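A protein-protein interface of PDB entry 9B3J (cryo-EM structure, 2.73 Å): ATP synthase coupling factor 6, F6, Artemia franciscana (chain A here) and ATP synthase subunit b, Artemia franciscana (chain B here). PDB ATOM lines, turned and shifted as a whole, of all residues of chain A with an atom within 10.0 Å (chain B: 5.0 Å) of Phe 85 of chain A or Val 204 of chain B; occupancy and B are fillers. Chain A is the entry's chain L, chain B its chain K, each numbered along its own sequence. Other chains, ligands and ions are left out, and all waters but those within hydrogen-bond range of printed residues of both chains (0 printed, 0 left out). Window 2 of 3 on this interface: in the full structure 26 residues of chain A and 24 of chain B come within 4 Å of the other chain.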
ATOM      1  N   LEU A  79     -17.077  10.066 -16.498  1.00  0.00           N
ATOM      2  CA  LEU A  79     -16.561   8.777 -16.058  1.00  0.00           C
ATOM      3  C   LEU A  79     -15.804   8.033 -17.148  1.00  0.00           C
ATOM      4  O   LEU A  79     -15.140   7.035 -16.846  1.00  0.00           O
ATOM      5  CB  LEU A  79     -17.707   7.902 -15.546  1.00  0.00           C
ATOM      6  CG  LEU A  79     -18.652   8.530 -14.520  1.00  0.00           C
ATOM      7  CD1 LEU A  79     -19.693   7.522 -14.054  1.00  0.00           C
ATOM      8  CD2 LEU A  79     -17.882   9.096 -13.337  1.00  0.00           C
ATOM      9  N   LYS A  81     -13.240   9.107 -18.713  1.00  0.00           N
ATOM     10  CA  LYS A  81     -11.841   9.495 -18.646  1.00  0.00           C
ATOM     11  C   LYS A  81     -11.241   9.057 -17.316  1.00  0.00           C
ATOM     12  O   LYS A  81     -11.936   8.579 -16.416  1.00  0.00           O
ATOM     13  CB  LYS A  81     -11.692  11.009 -18.830  1.00  0.00           C
ATOM     14  CG  LYS A  81     -12.342  11.537 -20.094  1.00  0.00           C
ATOM     15  CD  LYS A  81     -12.250  13.049 -20.169  1.00  0.00           C
ATOM     16  CE  LYS A  81     -12.913  13.578 -21.430  1.00  0.00           C
ATOM     17  NZ  LYS A  81     -12.851  15.063 -21.507  1.00  0.00           N
ATOM     18  N   PHE A  82      -9.929   9.225 -17.204  1.00  0.00           N
ATOM     19  CA  PHE A  82      -9.228   8.851 -15.984  1.00  0.00           C
ATOM     20  C   PHE A  82      -9.485   9.894 -14.904  1.00  0.00           C
ATOM     21  O   PHE A  82      -9.157  11.069 -15.103  1.00  0.00           O
ATOM     22  CB  PHE A  82      -7.734   8.721 -16.247  1.00  0.00           C
ATOM     23  CG  PHE A  82      -6.934   8.356 -15.031  1.00  0.00           C
ATOM     24  CD1 PHE A  82      -6.973   7.069 -14.523  1.00  0.00           C
ATOM     25  CD2 PHE A  82      -6.136   9.298 -14.400  1.00  0.00           C
ATOM     26  CE1 PHE A  82      -6.237   6.726 -13.402  1.00  0.00           C
ATOM     27  CE2 PHE A  82      -5.397   8.963 -13.279  1.00  0.00           C
ATOM     28  CZ  PHE A  82      -5.447   7.676 -12.780  1.00  0.00           C
ATOM     29  N   PRO A  83     -10.065   9.520 -13.766  1.00  0.00           N
ATOM     30  CA  PRO A  83     -10.325  10.507 -12.715  1.00  0.00           C
ATOM     31  C   PRO A  83      -9.051  10.927 -11.998  1.00  0.00           C
ATOM     32  O   PRO A  83      -8.064  10.192 -11.948  1.00  0.00           O
ATOM     33  CB  PRO A  83     -11.279   9.769 -11.768  1.00  0.00           C
ATOM     34  CG  PRO A  83     -10.954   8.330 -11.966  1.00  0.00           C
ATOM     35  CD  PRO A  83     -10.568   8.182 -13.411  1.00  0.00           C
ATOM     36  N   SER A  84      -9.090  12.132 -11.438  1.00  0.00           N
ATOM     37  CA  SER A  84      -7.998  12.673 -10.644  1.00  0.00           C
ATOM     38  C   SER A  84      -8.300  12.507  -9.160  1.00  0.00           C
ATOM     39  O   SER A  84      -9.462  12.482  -8.744  1.00  0.00           O
ATOM     40  CB  SER A  84      -7.767  14.151 -10.966  1.00  0.00           C
ATOM     41  OG  SER A  84      -8.921  14.921 -10.678  1.00  0.00           O
ATOM     42  N   PHE A  85      -7.242  12.396  -8.359  1.00  0.00           N
ATOM     43  CA  PHE A  85      -7.379  12.126  -6.936  1.00  0.00           C
ATOM     44  C   PHE A  85      -6.532  13.097  -6.127  1.00  0.00           C
ATOM     45  O   PHE A  85      -5.480  13.560  -6.580  1.00  0.00           O
ATOM     46  CB  PHE A  85      -6.973  10.686  -6.601  1.00  0.00           C
ATOM     47  CG  PHE A  85      -7.549   9.661  -7.535  1.00  0.00           C
ATOM     48  CD1 PHE A  85      -8.845   9.202  -7.370  1.00  0.00           C
ATOM     49  CD2 PHE A  85      -6.789   9.153  -8.578  1.00  0.00           C
ATOM     50  CE1 PHE A  85      -9.374   8.258  -8.226  1.00  0.00           C
ATOM     51  CE2 PHE A  85      -7.312   8.207  -9.439  1.00  0.00           C
ATOM     52  CZ  PHE A  85      -8.607   7.759  -9.261  1.00  0.00           C
ATOM     53  N   HIS A  86      -7.004  13.399  -4.919  1.00  0.00           N
ATOM     54  CA  HIS A  86      -6.292  14.268  -3.993  1.00  0.00           C
ATOM     55  C   HIS A  86      -6.202  13.585  -2.636  1.00  0.00           C
ATOM     56  O   HIS A  86      -7.224  13.175  -2.074  1.00  0.00           O
ATOM     57  CB  HIS A  86      -6.984  15.624  -3.861  1.00  0.00           C
ATOM     58  CG  HIS A  86      -6.187  16.639  -3.105  1.00  0.00           C
ATOM     59  ND1 HIS A  86      -6.472  16.989  -1.803  1.00  0.00           N
ATOM     60  CD2 HIS A  86      -5.117  17.383  -3.469  1.00  0.00           C
ATOM     61  CE1 HIS A  86      -5.612  17.905  -1.397  1.00  0.00           C
ATOM     62  NE2 HIS A  86      -4.779  18.162  -2.389  1.00  0.00           N
ATOM     63  N   PHE A  87      -4.976  13.481  -2.119  1.00  0.00           N
ATOM     64  CA  PHE A  87      -4.663  12.813  -0.858  1.00  0.00           C
ATOM     65  C   PHE A  87      -4.990  13.745   0.297  1.00  0.00           C
ATOM     66  O   PHE A  87      -4.348  14.784   0.462  1.00  0.00           O
ATOM     67  CB  PHE A  87      -3.194  12.422  -0.842  1.00  0.00           C
ATOM     68  CG  PHE A  87      -2.296  13.365  -1.616  1.00  0.00           C
ATOM     69  CD1 PHE A  87      -1.744  14.484  -1.014  1.00  0.00           C
ATOM     70  CD2 PHE A  87      -1.963  13.099  -2.931  1.00  0.00           C
ATOM     71  CE1 PHE A  87      -0.926  15.325  -1.706  1.00  0.00           C
ATOM     72  CE2 PHE A  87      -1.137  13.944  -3.626  1.00  0.00           C
ATOM     73  CZ  PHE A  87      -0.619  15.055  -3.012  1.00  0.00           C
ATOM     74  N   GLU A  88      -5.992  13.397   1.095  1.00  0.00           N
ATOM     75  CA  GLU A  88      -6.497  14.342   2.086  1.00  0.00           C
ATOM     76  C   GLU A  88      -5.479  14.494   3.202  1.00  0.00           C
ATOM     77  O   GLU A  88      -5.170  13.517   3.891  1.00  0.00           O
ATOM     78  CB  GLU A  88      -7.847  13.882   2.635  1.00  0.00           C
ATOM     79  CG  GLU A  88      -9.020  14.807   2.290  1.00  0.00           C
ATOM     80  CD  GLU A  88      -9.230  14.969   0.795  1.00  0.00           C
ATOM     81  OE1 GLU A  88      -9.327  13.943   0.087  1.00  0.00           O
ATOM     82  OE2 GLU A  88      -9.286  16.123   0.327  1.00  0.00           O
ATOM     83  N   ASP A  89      -4.971  15.715   3.372  1.00  0.00           N
ATOM     84  CA  ASP A  89      -3.764  15.958   4.149  1.00  0.00           C
ATOM     85  C   ASP A  89      -3.937  15.539   5.604  1.00  0.00           C
ATOM     86  O   ASP A  89      -4.853  16.031   6.279  1.00  0.00           O
ATOM     87  CB  ASP A  89      -3.367  17.421   4.057  1.00  0.00           C
ATOM     88  CG  ASP A  89      -2.479  17.693   2.867  1.00  0.00           C
ATOM     89  OD1 ASP A  89      -2.901  17.374   1.739  1.00  0.00           O
ATOM     90  OD2 ASP A  89      -1.357  18.205   3.058  1.00  0.00           O
ATOM     91  N   ALA B 199      -5.046   3.376   2.338  1.00  0.00           N
ATOM     92  CA  ALA B 199      -6.406   3.864   2.098  1.00  0.00           C
ATOM     93  C   ALA B 199      -6.510   4.669   0.812  1.00  0.00           C
ATOM     94  O   ALA B 199      -7.480   4.521   0.066  1.00  0.00           O
ATOM     95  CB  ALA B 199      -6.870   4.723   3.273  1.00  0.00           C
ATOM     96  N   ARG B 200      -5.548   5.558   0.548  1.00  0.00           N
ATOM     97  CA  ARG B 200      -5.582   6.272  -0.729  1.00  0.00           C
ATOM     98  C   ARG B 200      -5.291   5.354  -1.917  1.00  0.00           C
ATOM     99  O   ARG B 200      -5.804   5.595  -3.021  1.00  0.00           O
ATOM    100  CB  ARG B 200      -4.607   7.437  -0.726  1.00  0.00           C
ATOM    101  CG  ARG B 200      -4.868   8.427   0.365  1.00  0.00           C
ATOM    102  CD  ARG B 200      -6.301   8.916   0.369  1.00  0.00           C
ATOM    103  NE  ARG B 200      -6.517   9.966   1.361  1.00  0.00           N
ATOM    104  CZ  ARG B 200      -6.943   9.754   2.597  1.00  0.00           C
ATOM    105  NH1 ARG B 200      -7.238   8.539   3.027  1.00  0.00           N
ATOM    106  NH2 ARG B 200      -7.063  10.783   3.427  1.00  0.00           N
ATOM    107  N   LEU B 201      -4.504   4.288  -1.727  1.00  0.00           N
ATOM    108  CA  LEU B 201      -4.390   3.314  -2.806  1.00  0.00           C
ATOM    109  C   LEU B 201      -5.708   2.572  -3.019  1.00  0.00           C
ATOM    110  O   LEU B 201      -6.119   2.324  -4.163  1.00  0.00           O
ATOM    111  CB  LEU B 201      -3.254   2.334  -2.528  1.00  0.00           C
ATOM    112  CG  LEU B 201      -2.353   2.077  -3.758  1.00  0.00           C
ATOM    113  CD1 LEU B 201      -1.086   1.317  -3.409  1.00  0.00           C
ATOM    114  CD2 LEU B 201      -3.064   1.366  -4.913  1.00  0.00           C
ATOM    115  N   HIS B 202      -6.385   2.223  -1.926  1.00  0.00           N
ATOM    116  CA  HIS B 202      -7.679   1.548  -2.000  1.00  0.00           C
ATOM    117  C   HIS B 202      -8.723   2.437  -2.656  1.00  0.00           C
ATOM    118  O   HIS B 202      -9.551   1.958  -3.436  1.00  0.00           O
ATOM    119  CB  HIS B 202      -8.132   1.148  -0.595  1.00  0.00           C
ATOM    120  CG  HIS B 202      -9.131   0.038  -0.561  1.00  0.00           C
ATOM    121  ND1 HIS B 202     -10.036  -0.190  -1.574  1.00  0.00           N
ATOM    122  CD2 HIS B 202      -9.364  -0.915   0.373  1.00  0.00           C
ATOM    123  CE1 HIS B 202     -10.787  -1.232  -1.265  1.00  0.00           C
ATOM    124  NE2 HIS B 202     -10.398  -1.691  -0.089  1.00  0.00           N
ATOM    125  N   HIS B 203      -8.708   3.729  -2.332  1.00  0.00           N
ATOM    126  CA  HIS B 203      -9.665   4.663  -2.911  1.00  0.00           C
ATOM    127  C   HIS B 203      -9.454   4.801  -4.412  1.00  0.00           C
ATOM    128  O   HIS B 203     -10.427   4.849  -5.180  1.00  0.00           O
ATOM    129  CB  HIS B 203      -9.555   6.022  -2.223  1.00  0.00           C
ATOM    130  CG  HIS B 203     -10.705   6.937  -2.511  1.00  0.00           C
ATOM    131  ND1 HIS B 203     -11.839   6.518  -3.174  1.00  0.00           N
ATOM    132  CD2 HIS B 203     -10.896   8.246  -2.228  1.00  0.00           C
ATOM    133  CE1 HIS B 203     -12.679   7.531  -3.288  1.00  0.00           C
ATOM    134  NE2 HIS B 203     -12.131   8.592  -2.723  1.00  0.00           N
ATOM    135  N   VAL B 204      -8.188   4.843  -4.851  1.00  0.00           N
ATOM    136  CA  VAL B 204      -7.908   4.920  -6.284  1.00  0.00           C
ATOM    137  C   VAL B 204      -8.368   3.652  -7.007  1.00  0.00           C
ATOM    138  O   VAL B 204      -8.998   3.723  -8.077  1.00  0.00           O
ATOM    139  CB  VAL B 204      -6.411   5.199  -6.505  1.00  0.00           C
ATOM    140  CG1 VAL B 204      -6.026   4.982  -7.954  1.00  0.00           C
ATOM    141  CG2 VAL B 204      -6.088   6.621  -6.091  1.00  0.00           C
ATOM    142  N   ASN B 205      -8.078   2.479  -6.431  1.00  0.00           N
ATOM    143  CA  ASN B 205      -8.488   1.221  -7.059  1.00  0.00           C
ATOM    144  C   ASN B 205     -10.008   1.079  -7.100  1.00  0.00           C
ATOM    145  O   ASN B 205     -10.564   0.567  -8.082  1.00  0.00           O
ATOM    146  CB  ASN B 205      -7.862   0.038  -6.323  1.00  0.00           C
ATOM    147  CG  ASN B 205      -8.219  -1.297  -6.952  1.00  0.00           C
ATOM    148  OD1 ASN B 205      -7.593  -1.726  -7.921  1.00  0.00           O
ATOM    149  ND2 ASN B 205      -9.226  -1.964  -6.398  1.00  0.00           N
ATOM    150  N   ASN B 206     -10.696   1.526  -6.044  1.00  0.00           N
ATOM    151  CA  ASN B 206     -12.154   1.468  -6.020  1.00  0.00           C
ATOM    152  C   ASN B 206     -12.762   2.389  -7.071  1.00  0.00           C
ATOM    153  O   ASN B 206     -13.758   2.031  -7.713  1.00  0.00           O
ATOM    154  CB  ASN B 206     -12.665   1.830  -4.625  1.00  0.00           C
ATOM    155  CG  ASN B 206     -14.040   1.252  -4.337  1.00  0.00           C
ATOM    156  OD1 ASN B 206     -14.796   0.922  -5.249  1.00  0.00           O
ATOM    157  ND2 ASN B 206     -14.367   1.125  -3.057  1.00  0.00           N
ATOM    158  N   GLU B 207     -12.175   3.576  -7.261  1.00  0.00           N
ATOM    159  CA  GLU B 207     -12.671   4.482  -8.296  1.00  0.00           C
ATOM    160  C   GLU B 207     -12.461   3.909  -9.695  1.00  0.00           C
ATOM    161  O   GLU B 207     -13.336   4.044 -10.562  1.00  0.00           O
ATOM    162  CB  GLU B 207     -11.993   5.844  -8.167  1.00  0.00           C
ATOM    163  CG  GLU B 207     -12.465   6.662  -6.978  1.00  0.00           C
ATOM    164  CD  GLU B 207     -13.911   7.101  -7.106  1.00  0.00           C
ATOM    165  OE1 GLU B 207     -14.374   7.320  -8.246  1.00  0.00           O
ATOM    166  OE2 GLU B 207     -14.587   7.228  -6.063  1.00  0.00           O
ATOM    167  N   ILE B 208     -11.308   3.274  -9.932  1.00  0.00           N
ATOM    168  CA  ILE B 208     -11.047   2.661 -11.236  1.00  0.00           C
ATOM    169  C   ILE B 208     -12.023   1.515 -11.498  1.00  0.00           C
ATOM    170  O   ILE B 208     -12.548   1.364 -12.614  1.00  0.00           O
ATOM    171  CB  ILE B 208      -9.579   2.200 -11.318  1.00  0.00           C
ATOM    172  CG1 ILE B 208      -8.645   3.410 -11.328  1.00  0.00           C
ATOM    173  CG2 ILE B 208      -9.328   1.345 -12.554  1.00  0.00           C
ATOM    174  CD1 ILE B 208      -8.889   4.358 -12.481  1.00  0.00           C
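The guanidinium group of Arg 200 of chain B lies close to the backbone carbonyl oxygen of Glu 88 of chain A (3.4 Å).
Lys 81 of chain A touches none of the printed residues of chain B.
Of the printed residues of chain B, Phe 82 of chain A touches Ile 208.
Ser 84 of chain A touches none of the printed residues of chain B.
Printed residues of chain B within 4 Å of Phe 85 of chain A: Val 204 and Glu 207.
Printed residues of chain B within 4 Å of Glu 88 of chain A: Arg 200 (3.3 Å).
Printed residues of chain A within 4 Å of Arg 200 of chain B: Glu 88.
No residue of chain A comes within 4 Å of His 203 of chain B.
Of the printed residues of chain A, Val 204 of chain B touches Phe 85.
No residue of chain A comes within 4 Å of Asn 205 of chain B.
Printed residues of chain A within 4 Å of Glu 207 of chain B: Phe 85.
Of the printed residues of chain A, Ile 208 of chain B touches Phe 82.
Among the printed residues, pairs that only touch across the chains: Phe 82 of chain A with Ile 208 of chain B, Phe 85 of chain A with Val 204 of chain B and Phe 85 of chain A with Glu 207 of chain B.
Of the 10 printed residues of chain A, 3 touch a printed residue of chain B.
Hydrophobic or aromatic side chains of chain A within 4 Å of the printed part of chain B: Phe 82 and Phe 85.
Of the 10 printed residues of chain B, 4 touch a printed residue of chain A.
Hydrophobic or aromatic side chains of chain B that line the printed part of chain A: Val 204 and Ile 208.
Along chain B the printed residues that touch a printed residue of chain A span positions 200 to 208.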
